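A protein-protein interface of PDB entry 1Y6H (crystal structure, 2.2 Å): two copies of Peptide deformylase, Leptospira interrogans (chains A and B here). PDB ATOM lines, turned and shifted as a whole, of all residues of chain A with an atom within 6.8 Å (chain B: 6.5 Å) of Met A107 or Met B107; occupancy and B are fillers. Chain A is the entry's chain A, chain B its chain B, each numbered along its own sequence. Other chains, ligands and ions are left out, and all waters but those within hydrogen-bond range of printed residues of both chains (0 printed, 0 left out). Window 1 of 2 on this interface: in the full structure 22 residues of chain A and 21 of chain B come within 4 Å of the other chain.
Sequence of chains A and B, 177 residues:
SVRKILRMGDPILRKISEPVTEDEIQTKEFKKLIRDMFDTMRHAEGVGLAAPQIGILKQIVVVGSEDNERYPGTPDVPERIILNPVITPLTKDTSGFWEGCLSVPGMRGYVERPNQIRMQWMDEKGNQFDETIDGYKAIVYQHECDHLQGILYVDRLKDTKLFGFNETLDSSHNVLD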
ATOM      1  N   MET A   8     -13.153 -25.838 -17.348  1.00  0.00           N
ATOM      2  CA  MET A   8     -14.487 -25.623 -17.875  1.00  0.00           C
ATOM      3  C   MET A   8     -15.016 -24.296 -17.346  1.00  0.00           C
ATOM      4  O   MET A   8     -14.914 -23.992 -16.151  1.00  0.00           O
ATOM      5  CB  MET A   8     -15.406 -26.765 -17.461  1.00  0.00           C
ATOM      6  CG  MET A   8     -16.815 -26.637 -18.000  1.00  0.00           C
ATOM      7  SD  MET A   8     -17.726 -28.167 -17.800  1.00  0.00           S
ATOM      8  CE  MET A   8     -17.991 -28.170 -16.037  1.00  0.00           C
ATOM      9  N   GLU A  99     -15.779 -41.030 -18.469  1.00  0.00           N
ATOM     10  CA  GLU A  99     -14.748 -40.101 -18.882  1.00  0.00           C
ATOM     11  C   GLU A  99     -14.464 -38.980 -17.901  1.00  0.00           C
ATOM     12  O   GLU A  99     -15.311 -38.588 -17.093  1.00  0.00           O
ATOM     13  CB  GLU A  99     -15.107 -39.482 -20.228  1.00  0.00           C
ATOM     14  CG  GLU A  99     -14.922 -40.405 -21.410  1.00  0.00           C
ATOM     15  CD  GLU A  99     -15.366 -39.753 -22.699  1.00  0.00           C
ATOM     16  OE1 GLU A  99     -15.025 -38.564 -22.905  1.00  0.00           O
ATOM     17  OE2 GLU A  99     -16.047 -40.427 -23.502  1.00  0.00           O
ATOM     18  N   GLY A 100     -13.239 -38.479 -17.990  1.00  0.00           N
ATOM     19  CA  GLY A 100     -12.806 -37.365 -17.179  1.00  0.00           C
ATOM     20  C   GLY A 100     -12.141 -36.430 -18.171  1.00  0.00           C
ATOM     21  O   GLY A 100     -11.911 -36.804 -19.329  1.00  0.00           O
ATOM     22  N   CYS A 101     -11.827 -35.219 -17.737  1.00  0.00           N
ATOM     23  CA  CYS A 101     -11.188 -34.260 -18.610  1.00  0.00           C
ATOM     24  C   CYS A 101     -10.301 -33.358 -17.783  1.00  0.00           C
ATOM     25  O   CYS A 101     -10.696 -32.908 -16.708  1.00  0.00           O
ATOM     26  CB  CYS A 101     -12.237 -33.425 -19.334  1.00  0.00           C
ATOM     27  SG  CYS A 101     -11.535 -32.095 -20.338  1.00  0.00           S
ATOM     28  N   SER A 103      -9.698 -30.491 -18.237  1.00  0.00           N
ATOM     29  CA  SER A 103     -10.327 -29.181 -18.138  1.00  0.00           C
ATOM     30  C   SER A 103     -11.549 -29.221 -17.215  1.00  0.00           C
ATOM     31  O   SER A 103     -12.178 -28.195 -16.968  1.00  0.00           O
ATOM     32  CB  SER A 103     -10.733 -28.678 -19.524  1.00  0.00           C
ATOM     33  OG  SER A 103      -9.587 -28.362 -20.295  1.00  0.00           O
ATOM     34  N   VAL A 104     -11.880 -30.409 -16.715  1.00  0.00           N
ATOM     35  CA  VAL A 104     -13.006 -30.588 -15.799  1.00  0.00           C
ATOM     36  C   VAL A 104     -12.445 -31.404 -14.642  1.00  0.00           C
ATOM     37  O   VAL A 104     -12.851 -32.541 -14.396  1.00  0.00           O
ATOM     38  CB  VAL A 104     -14.170 -31.360 -16.466  1.00  0.00           C
ATOM     39  CG1 VAL A 104     -15.365 -31.437 -15.515  1.00  0.00           C
ATOM     40  CG2 VAL A 104     -14.580 -30.671 -17.753  1.00  0.00           C
ATOM     41  N   PRO A 105     -11.490 -30.820 -13.908  1.00  0.00           N
ATOM     42  CA  PRO A 105     -10.839 -31.473 -12.773  1.00  0.00           C
ATOM     43  C   PRO A 105     -11.739 -31.943 -11.631  1.00  0.00           C
ATOM     44  O   PRO A 105     -12.666 -31.249 -11.220  1.00  0.00           O
ATOM     45  CB  PRO A 105      -9.825 -30.424 -12.322  1.00  0.00           C
ATOM     46  CG  PRO A 105     -10.530 -29.144 -12.626  1.00  0.00           C
ATOM     47  CD  PRO A 105     -11.072 -29.407 -14.004  1.00  0.00           C
ATOM     48  N   GLY A 106     -11.448 -33.143 -11.133  1.00  0.00           N
ATOM     49  CA  GLY A 106     -12.181 -33.704 -10.014  1.00  0.00           C
ATOM     50  C   GLY A 106     -13.515 -34.346 -10.314  1.00  0.00           C
ATOM     51  O   GLY A 106     -14.248 -34.706  -9.401  1.00  0.00           O
ATOM     52  N   MET A 107     -13.839 -34.507 -11.589  1.00  0.00           N
ATOM     53  CA  MET A 107     -15.112 -35.106 -11.940  1.00  0.00           C
ATOM     54  C   MET A 107     -15.004 -36.113 -13.059  1.00  0.00           C
ATOM     55  O   MET A 107     -13.952 -36.287 -13.675  1.00  0.00           O
ATOM     56  CB  MET A 107     -16.093 -34.029 -12.383  1.00  0.00           C
ATOM     57  CG  MET A 107     -16.170 -32.825 -11.464  1.00  0.00           C
ATOM     58  SD  MET A 107     -17.538 -31.739 -11.936  1.00  0.00           S
ATOM     59  CE  MET A 107     -16.734 -30.526 -12.797  1.00  0.00           C
ATOM     60  N   ARG A 108     -16.122 -36.775 -13.312  1.00  0.00           N
ATOM     61  CA  ARG A 108     -16.208 -37.717 -14.398  1.00  0.00           C
ATOM     62  C   ARG A 108     -17.663 -38.001 -14.692  1.00  0.00           C
ATOM     63  O   ARG A 108     -18.542 -37.811 -13.845  1.00  0.00           O
ATOM     64  CB  ARG A 108     -15.411 -38.993 -14.117  1.00  0.00           C
ATOM     65  CG  ARG A 108     -15.720 -39.738 -12.852  1.00  0.00           C
ATOM     66  CD  ARG A 108     -14.825 -40.976 -12.810  1.00  0.00           C
ATOM     67  NE  ARG A 108     -15.157 -41.867 -11.706  1.00  0.00           N
ATOM     68  CZ  ARG A 108     -14.580 -41.827 -10.511  1.00  0.00           C
ATOM     69  NH1 ARG A 108     -13.632 -40.935 -10.259  1.00  0.00           N
ATOM     70  NH2 ARG A 108     -14.954 -42.684  -9.572  1.00  0.00           N
ATOM     71  N   GLY A 109     -17.916 -38.414 -15.922  1.00  0.00           N
ATOM     72  CA  GLY A 109     -19.273 -38.671 -16.333  1.00  0.00           C
ATOM     73  C   GLY A 109     -19.327 -39.780 -17.342  1.00  0.00           C
ATOM     74  O   GLY A 109     -18.364 -40.034 -18.076  1.00  0.00           O
ATOM     75  N   TYR A 153     -16.803 -33.252 -22.754  1.00  0.00           N
ATOM     76  CA  TYR A 153     -17.606 -34.455 -22.563  1.00  0.00           C
ATOM     77  C   TYR A 153     -18.896 -34.196 -21.792  1.00  0.00           C
ATOM     78  O   TYR A 153     -19.855 -34.962 -21.915  1.00  0.00           O
ATOM     79  CB  TYR A 153     -16.784 -35.546 -21.873  1.00  0.00           C
ATOM     80  CG  TYR A 153     -16.621 -35.366 -20.382  1.00  0.00           C
ATOM     81  CD1 TYR A 153     -17.550 -35.904 -19.485  1.00  0.00           C
ATOM     82  CD2 TYR A 153     -15.530 -34.670 -19.864  1.00  0.00           C
ATOM     83  CE1 TYR A 153     -17.390 -35.753 -18.104  1.00  0.00           C
ATOM     84  CE2 TYR A 153     -15.363 -34.512 -18.499  1.00  0.00           C
ATOM     85  CZ  TYR A 153     -16.287 -35.054 -17.622  1.00  0.00           C
ATOM     86  OH  TYR A 153     -16.079 -34.912 -16.268  1.00  0.00           O
ATOM     87  N   VAL A 154     -18.932 -33.122 -21.007  1.00  0.00           N
ATOM     88  CA  VAL A 154     -20.144 -32.819 -20.250  1.00  0.00           C
ATOM     89  C   VAL A 154     -21.266 -32.491 -21.222  1.00  0.00           C
ATOM     90  O   VAL A 154     -22.439 -32.551 -20.871  1.00  0.00           O
ATOM     91  CB  VAL A 154     -19.945 -31.633 -19.275  1.00  0.00           C
ATOM     92  CG1 VAL A 154     -18.888 -31.990 -18.245  1.00  0.00           C
ATOM     93  CG2 VAL A 154     -19.543 -30.383 -20.036  1.00  0.00           C
ATOM     94  N   PHE A 163     -22.897 -38.543 -13.334  1.00  0.00           N
ATOM     95  CA  PHE A 163     -21.906 -37.486 -13.386  1.00  0.00           C
ATOM     96  C   PHE A 163     -21.690 -37.030 -11.949  1.00  0.00           C
ATOM     97  O   PHE A 163     -22.639 -36.954 -11.171  1.00  0.00           O
ATOM     98  CB  PHE A 163     -22.484 -36.355 -14.245  1.00  0.00           C
ATOM     99  CG  PHE A 163     -21.601 -35.153 -14.375  1.00  0.00           C
ATOM    100  CD1 PHE A 163     -20.261 -35.280 -14.721  1.00  0.00           C
ATOM    101  CD2 PHE A 163     -22.134 -33.875 -14.218  1.00  0.00           C
ATOM    102  CE1 PHE A 163     -19.460 -34.153 -14.913  1.00  0.00           C
ATOM    103  CE2 PHE A 163     -21.342 -32.740 -14.408  1.00  0.00           C
ATOM    104  CZ  PHE A 163     -20.000 -32.883 -14.758  1.00  0.00           C
ATOM    105  N   GLY A 164     -20.449 -36.742 -11.583  1.00  0.00           N
ATOM    106  CA  GLY A 164     -20.197 -36.307 -10.226  1.00  0.00           C
ATOM    107  C   GLY A 164     -18.727 -36.175  -9.919  1.00  0.00           C
ATOM    108  O   GLY A 164     -17.889 -36.248 -10.818  1.00  0.00           O
ATOM    109  N   PHE A 165     -18.410 -35.976  -8.645  1.00  0.00           N
ATOM    110  CA  PHE A 165     -17.023 -35.839  -8.246  1.00  0.00           C
ATOM    111  C   PHE A 165     -16.392 -37.185  -8.002  1.00  0.00           C
ATOM    112  O   PHE A 165     -17.004 -38.080  -7.423  1.00  0.00           O
ATOM    113  CB  PHE A 165     -16.916 -34.966  -7.007  1.00  0.00           C
ATOM    114  CG  PHE A 165     -17.460 -33.596  -7.214  1.00  0.00           C
ATOM    115  CD1 PHE A 165     -18.823 -33.362  -7.118  1.00  0.00           C
ATOM    116  CD2 PHE A 165     -16.616 -32.543  -7.559  1.00  0.00           C
ATOM    117  CE1 PHE A 165     -19.352 -32.102  -7.362  1.00  0.00           C
ATOM    118  CE2 PHE A 165     -17.136 -31.267  -7.808  1.00  0.00           C
ATOM    119  CZ  PHE A 165     -18.507 -31.046  -7.709  1.00  0.00           C
ATOM    120  N   ASN A 166     -15.155 -37.309  -8.455  1.00  0.00           N
ATOM    121  CA  ASN A 166     -14.419 -38.548  -8.331  1.00  0.00           C
ATOM    122  C   ASN A 166     -14.480 -39.183  -6.961  1.00  0.00           C
ATOM    123  O   ASN A 166     -14.886 -40.332  -6.825  1.00  0.00           O
ATOM    124  CB  ASN A 166     -12.974 -38.306  -8.739  1.00  0.00           C
ATOM    125  CG  ASN A 166     -12.874 -37.736 -10.123  1.00  0.00           C
ATOM    126  OD1 ASN A 166     -13.610 -38.149 -11.020  1.00  0.00           O
ATOM    127  ND2 ASN A 166     -11.968 -36.789 -10.316  1.00  0.00           N
ATOM    128  N   LEU A 169     -18.035 -40.239  -6.158  1.00  0.00           N
ATOM    129  CA  LEU A 169     -18.394 -41.395  -6.971  1.00  0.00           C
ATOM    130  C   LEU A 169     -17.644 -42.641  -6.488  1.00  0.00           C
ATOM    131  O   LEU A 169     -18.212 -43.731  -6.448  1.00  0.00           O
ATOM    132  CB  LEU A 169     -18.071 -41.132  -8.447  1.00  0.00           C
ATOM    133  CG  LEU A 169     -18.941 -40.090  -9.152  1.00  0.00           C
ATOM    134  CD1 LEU A 169     -18.358 -39.739 -10.504  1.00  0.00           C
ATOM    135  CD2 LEU A 169     -20.364 -40.633  -9.303  1.00  0.00           C
ATOM    136  N   MET B   8     -22.516 -33.942  -5.554  1.00  0.00           N
ATOM    137  CA  MET B   8     -23.071 -34.570  -6.739  1.00  0.00           C
ATOM    138  C   MET B   8     -22.318 -35.866  -6.979  1.00  0.00           C
ATOM    139  O   MET B   8     -21.090 -35.906  -6.906  1.00  0.00           O
ATOM    140  CB  MET B   8     -22.939 -33.640  -7.941  1.00  0.00           C
ATOM    141  CG  MET B   8     -23.490 -34.216  -9.228  1.00  0.00           C
ATOM    142  SD  MET B   8     -23.607 -32.962 -10.502  1.00  0.00           S
ATOM    143  CE  MET B   8     -21.932 -32.723 -10.904  1.00  0.00           C
ATOM    144  N   ARG B  70     -21.620 -15.913  -1.832  1.00  0.00           N
ATOM    145  CA  ARG B  70     -21.626 -16.850  -2.952  1.00  0.00           C
ATOM    146  C   ARG B  70     -22.432 -16.329  -4.144  1.00  0.00           C
ATOM    147  O   ARG B  70     -22.206 -16.754  -5.271  1.00  0.00           O
ATOM    148  CB  ARG B  70     -22.165 -18.213  -2.507  1.00  0.00           C
ATOM    149  CG  ARG B  70     -21.143 -19.104  -1.793  1.00  0.00           C
ATOM    150  CD  ARG B  70     -21.640 -20.544  -1.804  1.00  0.00           C
ATOM    151  NE  ARG B  70     -22.463 -20.764  -2.995  1.00  0.00           N
ATOM    152  CZ  ARG B  70     -23.099 -21.894  -3.297  1.00  0.00           C
ATOM    153  NH1 ARG B  70     -23.822 -21.970  -4.405  1.00  0.00           N
ATOM    154  NH2 ARG B  70     -23.011 -22.948  -2.507  1.00  0.00           N
ATOM    155  N   TYR B  71     -23.373 -15.422  -3.892  1.00  0.00           N
ATOM    156  CA  TYR B  71     -24.191 -14.824  -4.957  1.00  0.00           C
ATOM    157  C   TYR B  71     -24.311 -13.335  -4.668  1.00  0.00           C
ATOM    158  O   TYR B  71     -25.392 -12.841  -4.341  1.00  0.00           O
ATOM    159  CB  TYR B  71     -25.594 -15.430  -5.002  1.00  0.00           C
ATOM    160  CG  TYR B  71     -25.622 -16.923  -5.184  1.00  0.00           C
ATOM    161  CD1 TYR B  71     -25.581 -17.775  -4.081  1.00  0.00           C
ATOM    162  CD2 TYR B  71     -25.680 -17.488  -6.455  1.00  0.00           C
ATOM    163  CE1 TYR B  71     -25.599 -19.152  -4.238  1.00  0.00           C
ATOM    164  CE2 TYR B  71     -25.696 -18.865  -6.623  1.00  0.00           C
ATOM    165  CZ  TYR B  71     -25.656 -19.693  -5.509  1.00  0.00           C
ATOM    166  OH  TYR B  71     -25.682 -21.059  -5.664  1.00  0.00           O
ATOM    167  N   GLU B  99     -26.755 -20.290 -11.487  1.00  0.00           N
ATOM    168  CA  GLU B  99     -26.929 -20.973 -10.223  1.00  0.00           C
ATOM    169  C   GLU B  99     -25.732 -21.790  -9.770  1.00  0.00           C
ATOM    170  O   GLU B  99     -24.901 -22.228 -10.569  1.00  0.00           O
ATOM    171  CB  GLU B  99     -28.155 -21.892 -10.295  1.00  0.00           C
ATOM    172  CG  GLU B  99     -29.491 -21.176 -10.203  1.00  0.00           C
ATOM    173  CD  GLU B  99     -30.668 -22.126 -10.338  1.00  0.00           C
ATOM    174  OE1 GLU B  99     -30.644 -23.216  -9.723  1.00  0.00           O
ATOM    175  OE2 GLU B  99     -31.624 -21.781 -11.058  1.00  0.00           O
ATOM    176  N   GLY B 100     -25.668 -21.976  -8.462  1.00  0.00           N
ATOM    177  CA  GLY B 100     -24.633 -22.778  -7.855  1.00  0.00           C
ATOM    178  C   GLY B 100     -25.378 -23.694  -6.904  1.00  0.00           C
ATOM    179  O   GLY B 100     -26.586 -23.536  -6.707  1.00  0.00           O
ATOM    180  N   CYS B 101     -24.681 -24.654  -6.317  1.00  0.00           N
ATOM    181  CA  CYS B 101     -25.313 -25.565  -5.382  1.00  0.00           C
ATOM    182  C   CYS B 101     -24.285 -26.069  -4.390  1.00  0.00           C
ATOM    183  O   CYS B 101     -23.184 -26.461  -4.767  1.00  0.00           O
ATOM    184  CB  CYS B 101     -25.937 -26.749  -6.121  1.00  0.00           C
ATOM    185  SG  CYS B 101     -26.699 -27.979  -5.018  1.00  0.00           S
ATOM    186  N   VAL B 104     -22.760 -29.060  -5.330  1.00  0.00           N
ATOM    187  CA  VAL B 104     -21.957 -29.021  -6.554  1.00  0.00           C
ATOM    188  C   VAL B 104     -20.945 -27.900  -6.323  1.00  0.00           C
ATOM    189  O   VAL B 104     -20.936 -26.891  -7.022  1.00  0.00           O
ATOM    190  CB  VAL B 104     -22.816 -28.690  -7.796  1.00  0.00           C
ATOM    191  CG1 VAL B 104     -21.972 -28.771  -9.045  1.00  0.00           C
ATOM    192  CG2 VAL B 104     -23.983 -29.658  -7.899  1.00  0.00           C
ATOM    193  N   PRO B 105     -20.072 -28.076  -5.323  1.00  0.00           N
ATOM    194  CA  PRO B 105     -19.053 -27.089  -4.966  1.00  0.00           C
ATOM    195  C   PRO B 105     -18.085 -26.676  -6.071  1.00  0.00           C
ATOM    196  O   PRO B 105     -17.619 -27.506  -6.857  1.00  0.00           O
ATOM    197  CB  PRO B 105     -18.349 -27.750  -3.779  1.00  0.00           C
ATOM    198  CG  PRO B 105     -18.421 -29.192  -4.127  1.00  0.00           C
ATOM    199  CD  PRO B 105     -19.847 -29.339  -4.597  1.00  0.00           C
ATOM    200  N   GLY B 106     -17.816 -25.374  -6.123  1.00  0.00           N
ATOM    201  CA  GLY B 106     -16.880 -24.816  -7.083  1.00  0.00           C
ATOM    202  C   GLY B 106     -17.368 -24.609  -8.496  1.00  0.00           C
ATOM    203  O   GLY B 106     -16.572 -24.306  -9.387  1.00  0.00           O
ATOM    204  N   MET B 107     -18.668 -24.763  -8.713  1.00  0.00           N
ATOM    205  CA  MET B 107     -19.211 -24.597 -10.050  1.00  0.00           C
ATOM    206  C   MET B 107     -20.445 -23.711 -10.109  1.00  0.00           C
ATOM    207  O   MET B 107     -21.059 -23.409  -9.086  1.00  0.00           O
ATOM    208  CB  MET B 107     -19.532 -25.960 -10.645  1.00  0.00           C
ATOM    209  CG  MET B 107     -18.377 -26.938 -10.567  1.00  0.00           C
ATOM    210  SD  MET B 107     -18.736 -28.352 -11.572  1.00  0.00           S
ATOM    211  CE  MET B 107     -19.233 -29.498 -10.385  1.00  0.00           C
ATOM    212  N   ARG B 108     -20.790 -23.294 -11.323  1.00  0.00           N
ATOM    213  CA  ARG B 108     -21.948 -22.450 -11.580  1.00  0.00           C
ATOM    214  C   ARG B 108     -22.478 -22.837 -12.958  1.00  0.00           C
ATOM    215  O   ARG B 108     -21.726 -23.244 -13.835  1.00  0.00           O
ATOM    216  CB  ARG B 108     -21.536 -20.972 -11.565  1.00  0.00           C
ATOM    217  CG  ARG B 108     -22.224 -20.098 -10.515  1.00  0.00           C
ATOM    218  CD  ARG B 108     -22.159 -20.735  -9.150  1.00  0.00           C
ATOM    219  NE  ARG B 108     -21.903 -19.775  -8.085  1.00  0.00           N
ATOM    220  CZ  ARG B 108     -21.475 -20.122  -6.874  1.00  0.00           C
ATOM    221  NH1 ARG B 108     -21.257 -19.196  -5.947  1.00  0.00           N
ATOM    222  NH2 ARG B 108     -21.259 -21.403  -6.591  1.00  0.00           N
ATOM    223  N   GLY B 109     -23.783 -22.732 -13.144  1.00  0.00           N
ATOM    224  CA  GLY B 109     -24.360 -23.067 -14.425  1.00  0.00           C
ATOM    225  C   GLY B 109     -25.551 -22.179 -14.674  1.00  0.00           C
ATOM    226  O   GLY B 109     -26.273 -21.823 -13.742  1.00  0.00           O
ATOM    227  N   TYR B 153     -29.466 -28.703 -10.188  1.00  0.00           N
ATOM    228  CA  TYR B 153     -29.552 -27.721 -11.271  1.00  0.00           C
ATOM    229  C   TYR B 153     -28.809 -28.164 -12.528  1.00  0.00           C
ATOM    230  O   TYR B 153     -29.123 -27.714 -13.633  1.00  0.00           O
ATOM    231  CB  TYR B 153     -29.028 -26.358 -10.801  1.00  0.00           C
ATOM    232  CG  TYR B 153     -27.524 -26.230 -10.758  1.00  0.00           C
ATOM    233  CD1 TYR B 153     -26.805 -25.811 -11.883  1.00  0.00           C
ATOM    234  CD2 TYR B 153     -26.820 -26.502  -9.590  1.00  0.00           C
ATOM    235  CE1 TYR B 153     -25.417 -25.658 -11.834  1.00  0.00           C
ATOM    236  CE2 TYR B 153     -25.440 -26.354  -9.531  1.00  0.00           C
ATOM    237  CZ  TYR B 153     -24.743 -25.928 -10.651  1.00  0.00           C
ATOM    238  OH  TYR B 153     -23.377 -25.741 -10.573  1.00  0.00           O
ATOM    239  N   VAL B 154     -27.821 -29.040 -12.374  1.00  0.00           N
ATOM    240  CA  VAL B 154     -27.096 -29.500 -13.549  1.00  0.00           C
ATOM    241  C   VAL B 154     -28.053 -30.250 -14.465  1.00  0.00           C
ATOM    242  O   VAL B 154     -27.796 -30.384 -15.657  1.00  0.00           O
ATOM    243  CB  VAL B 154     -25.902 -30.417 -13.178  1.00  0.00           C
ATOM    244  CG1 VAL B 154     -24.897 -29.640 -12.348  1.00  0.00           C
ATOM    245  CG2 VAL B 154     -26.389 -31.636 -12.415  1.00  0.00           C
ATOM    246  N   PHE B 163     -21.583 -23.530 -18.244  1.00  0.00           N
ATOM    247  CA  PHE B 163     -21.381 -24.296 -17.033  1.00  0.00           C
ATOM    248  C   PHE B 163     -19.870 -24.409 -16.869  1.00  0.00           C
ATOM    249  O   PHE B 163     -19.152 -24.582 -17.847  1.00  0.00           O
ATOM    250  CB  PHE B 163     -22.026 -25.672 -17.246  1.00  0.00           C
ATOM    251  CG  PHE B 163     -21.873 -26.621 -16.096  1.00  0.00           C
ATOM    252  CD1 PHE B 163     -22.161 -26.219 -14.793  1.00  0.00           C
ATOM    253  CD2 PHE B 163     -21.500 -27.945 -16.329  1.00  0.00           C
ATOM    254  CE1 PHE B 163     -22.084 -27.124 -13.732  1.00  0.00           C
ATOM    255  CE2 PHE B 163     -21.419 -28.862 -15.278  1.00  0.00           C
ATOM    256  CZ  PHE B 163     -21.713 -28.451 -13.977  1.00  0.00           C
ATOM    257  N   GLY B 164     -19.378 -24.298 -15.643  1.00  0.00           N
ATOM    258  CA  GLY B 164     -17.944 -24.403 -15.449  1.00  0.00           C
ATOM    259  C   GLY B 164     -17.549 -24.115 -14.024  1.00  0.00           C
ATOM    260  O   GLY B 164     -18.404 -24.009 -13.146  1.00  0.00           O
ATOM    261  N   PHE B 165     -16.252 -23.983 -13.784  1.00  0.00           N
ATOM    262  CA  PHE B 165     -15.782 -23.716 -12.437  1.00  0.00           C
ATOM    263  C   PHE B 165     -15.802 -22.218 -12.125  1.00  0.00           C
ATOM    264  O   PHE B 165     -15.409 -21.397 -12.952  1.00  0.00           O
ATOM    265  CB  PHE B 165     -14.391 -24.328 -12.251  1.00  0.00           C
ATOM    266  CG  PHE B 165     -14.363 -25.820 -12.464  1.00  0.00           C
ATOM    267  CD1 PHE B 165     -14.274 -26.355 -13.743  1.00  0.00           C
ATOM    268  CD2 PHE B 165     -14.461 -26.688 -11.379  1.00  0.00           C
ATOM    269  CE1 PHE B 165     -14.282 -27.736 -13.941  1.00  0.00           C
ATOM    270  CE2 PHE B 165     -14.471 -28.070 -11.566  1.00  0.00           C
ATOM    271  CZ  PHE B 165     -14.381 -28.595 -12.847  1.00  0.00           C
ATOM    272  N   ASN B 166     -16.286 -21.879 -10.927  1.00  0.00           N
ATOM    273  CA  ASN B 166     -16.423 -20.494 -10.457  1.00  0.00           C
ATOM    274  C   ASN B 166     -15.219 -19.576 -10.617  1.00  0.00           C
ATOM    275  O   ASN B 166     -15.365 -18.406 -10.982  1.00  0.00           O
ATOM    276  CB  ASN B 166     -16.818 -20.461  -8.981  1.00  0.00           C
ATOM    277  CG  ASN B 166     -18.065 -21.245  -8.698  1.00  0.00           C
ATOM    278  OD1 ASN B 166     -18.987 -21.289  -9.514  1.00  0.00           O
ATOM    279  ND2 ASN B 166     -18.114 -21.865  -7.528  1.00  0.00           N
ATOM    280  N   LEU B 169     -15.156 -18.820 -14.155  1.00  0.00           N
ATOM    281  CA  LEU B 169     -16.384 -18.110 -14.497  1.00  0.00           C
ATOM    282  C   LEU B 169     -16.387 -16.691 -13.952  1.00  0.00           C
ATOM    283  O   LEU B 169     -17.068 -15.824 -14.489  1.00  0.00           O
ATOM    284  CB  LEU B 169     -17.610 -18.855 -13.969  1.00  0.00           C
ATOM    285  CG  LEU B 169     -18.015 -20.135 -14.703  1.00  0.00           C
ATOM    286  CD1 LEU B 169     -19.240 -20.734 -14.019  1.00  0.00           C
ATOM    287  CD2 LEU B 169     -18.311 -19.835 -16.154  1.00  0.00           C
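Met A107 touches two residues of chain B.
Printed residues of chain A within 4 Å of Pro B105: Phe A165.
Of the printed residues of chain B, Met A8 touches Phe B163 (3.1 Å), Gly B164 (3.1 Å) and Phe B165 (2.7 Å).
Of the printed residues of chain B, Gly A164 touches Met B8 (3.5 Å).
Printed residues of chain A within 4 Å of Phe B165: Met A8, Ser A103, Val A104, Pro A105 and Met A107.
Of the printed residues of chain B, Ser A103 touches Phe B165.
Arg B70 touches none of the printed residues of chain A.
The nearest printed residue of chain A that does not touch Pro B105 is Met A107 (6.6 Å).
The backbone NH of Phe B165 sits at hydrogen-bond distance from the backbone carbonyl oxygen of Met A8 (2.7 Å).
N of Phe A165 sits at hydrogen-bond distance from O of Met B8.
The side-chain sulfur (SD) of Met A107 lies close to the side-chain sulfur (SD) of Met B107 (3.6 Å).
O of Ser A103 is in hydrogen-bond range of N of Met A8, at 2.6 Å.
The side-chain sulfur of Cys A101 sits close to the backbone NH of Ser A103 (3.2 Å).
N of Met A107 sits close to ND2 of Asn A166 (3.2 Å).
The backbone NH (N) of Arg A108 is in hydrogen-bond range of the backbone carbonyl oxygen (O) of Gly A164 (3.1 Å).
The backbone carbonyl oxygen (O) of Met B107 sits close to the side-chain amide oxygen (OD1) of Asn B166, at 3.0 Å.
N of Arg B108 is in hydrogen-bond range of O of Gly B164 (3.1 Å).
Printed residues of chain A that touch a printed residue of chain B: Met A8, Ser A103, Val A104, Pro A105, Met A107, Phe A163, Gly A164 and Phe A165.
Hydrophobic or aromatic side chains of chain A that line the printed part of chain B: Met A8, Pro A105, Met A107, Phe A163 and Phe A165.
Hydrophobic or aromatic side chains of chain B within 4 Å of the printed part of chain A: Met B8, Pro B105, Met B107, Phe B163 and Phe B165.
Met A8 touches Phe B163 (CG to O, 3.1 Å).
CA of Gly B164 touches O of Met A8, at 3.1 Å.
O of Ser A103 touches CE1 of Phe B165 (3.7 Å).
CE1 of Phe B165 touches CA of Val A104, 3.6 Å away.
Pro A105 touches Phe B165 (O to CZ, 3.6 Å).
CE of Met A107 touches CZ of Phe B165 (3.0 Å).
Met B8 touches Phe A163.
Phe A163 touches Phe B163.
Met B8 touches Gly A164 (O to CA, 3.5 Å).
Phe A165 touches Met B107 (CZ to CE, 3.2 Å).
Met A8 touches Phe B163, and with the chains exchanged Phe A163 touches Met B8.
Met A8 touches Phe B165, and with the chains exchanged Phe A165 touches Met B8.
Val A104 touches Phe B165, but with the chains exchanged Phe A165 does not touch Val B104 (4.1 Å).
Pro A105 touches Phe B165, and with the chains exchanged Phe A165 touches Pro B105.
Positions printed for both chains: 8, 99, 100, 101, 104, 105, 106, 107, 108, 109, 153, 154, 163, 164, 165, 166 and 169.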
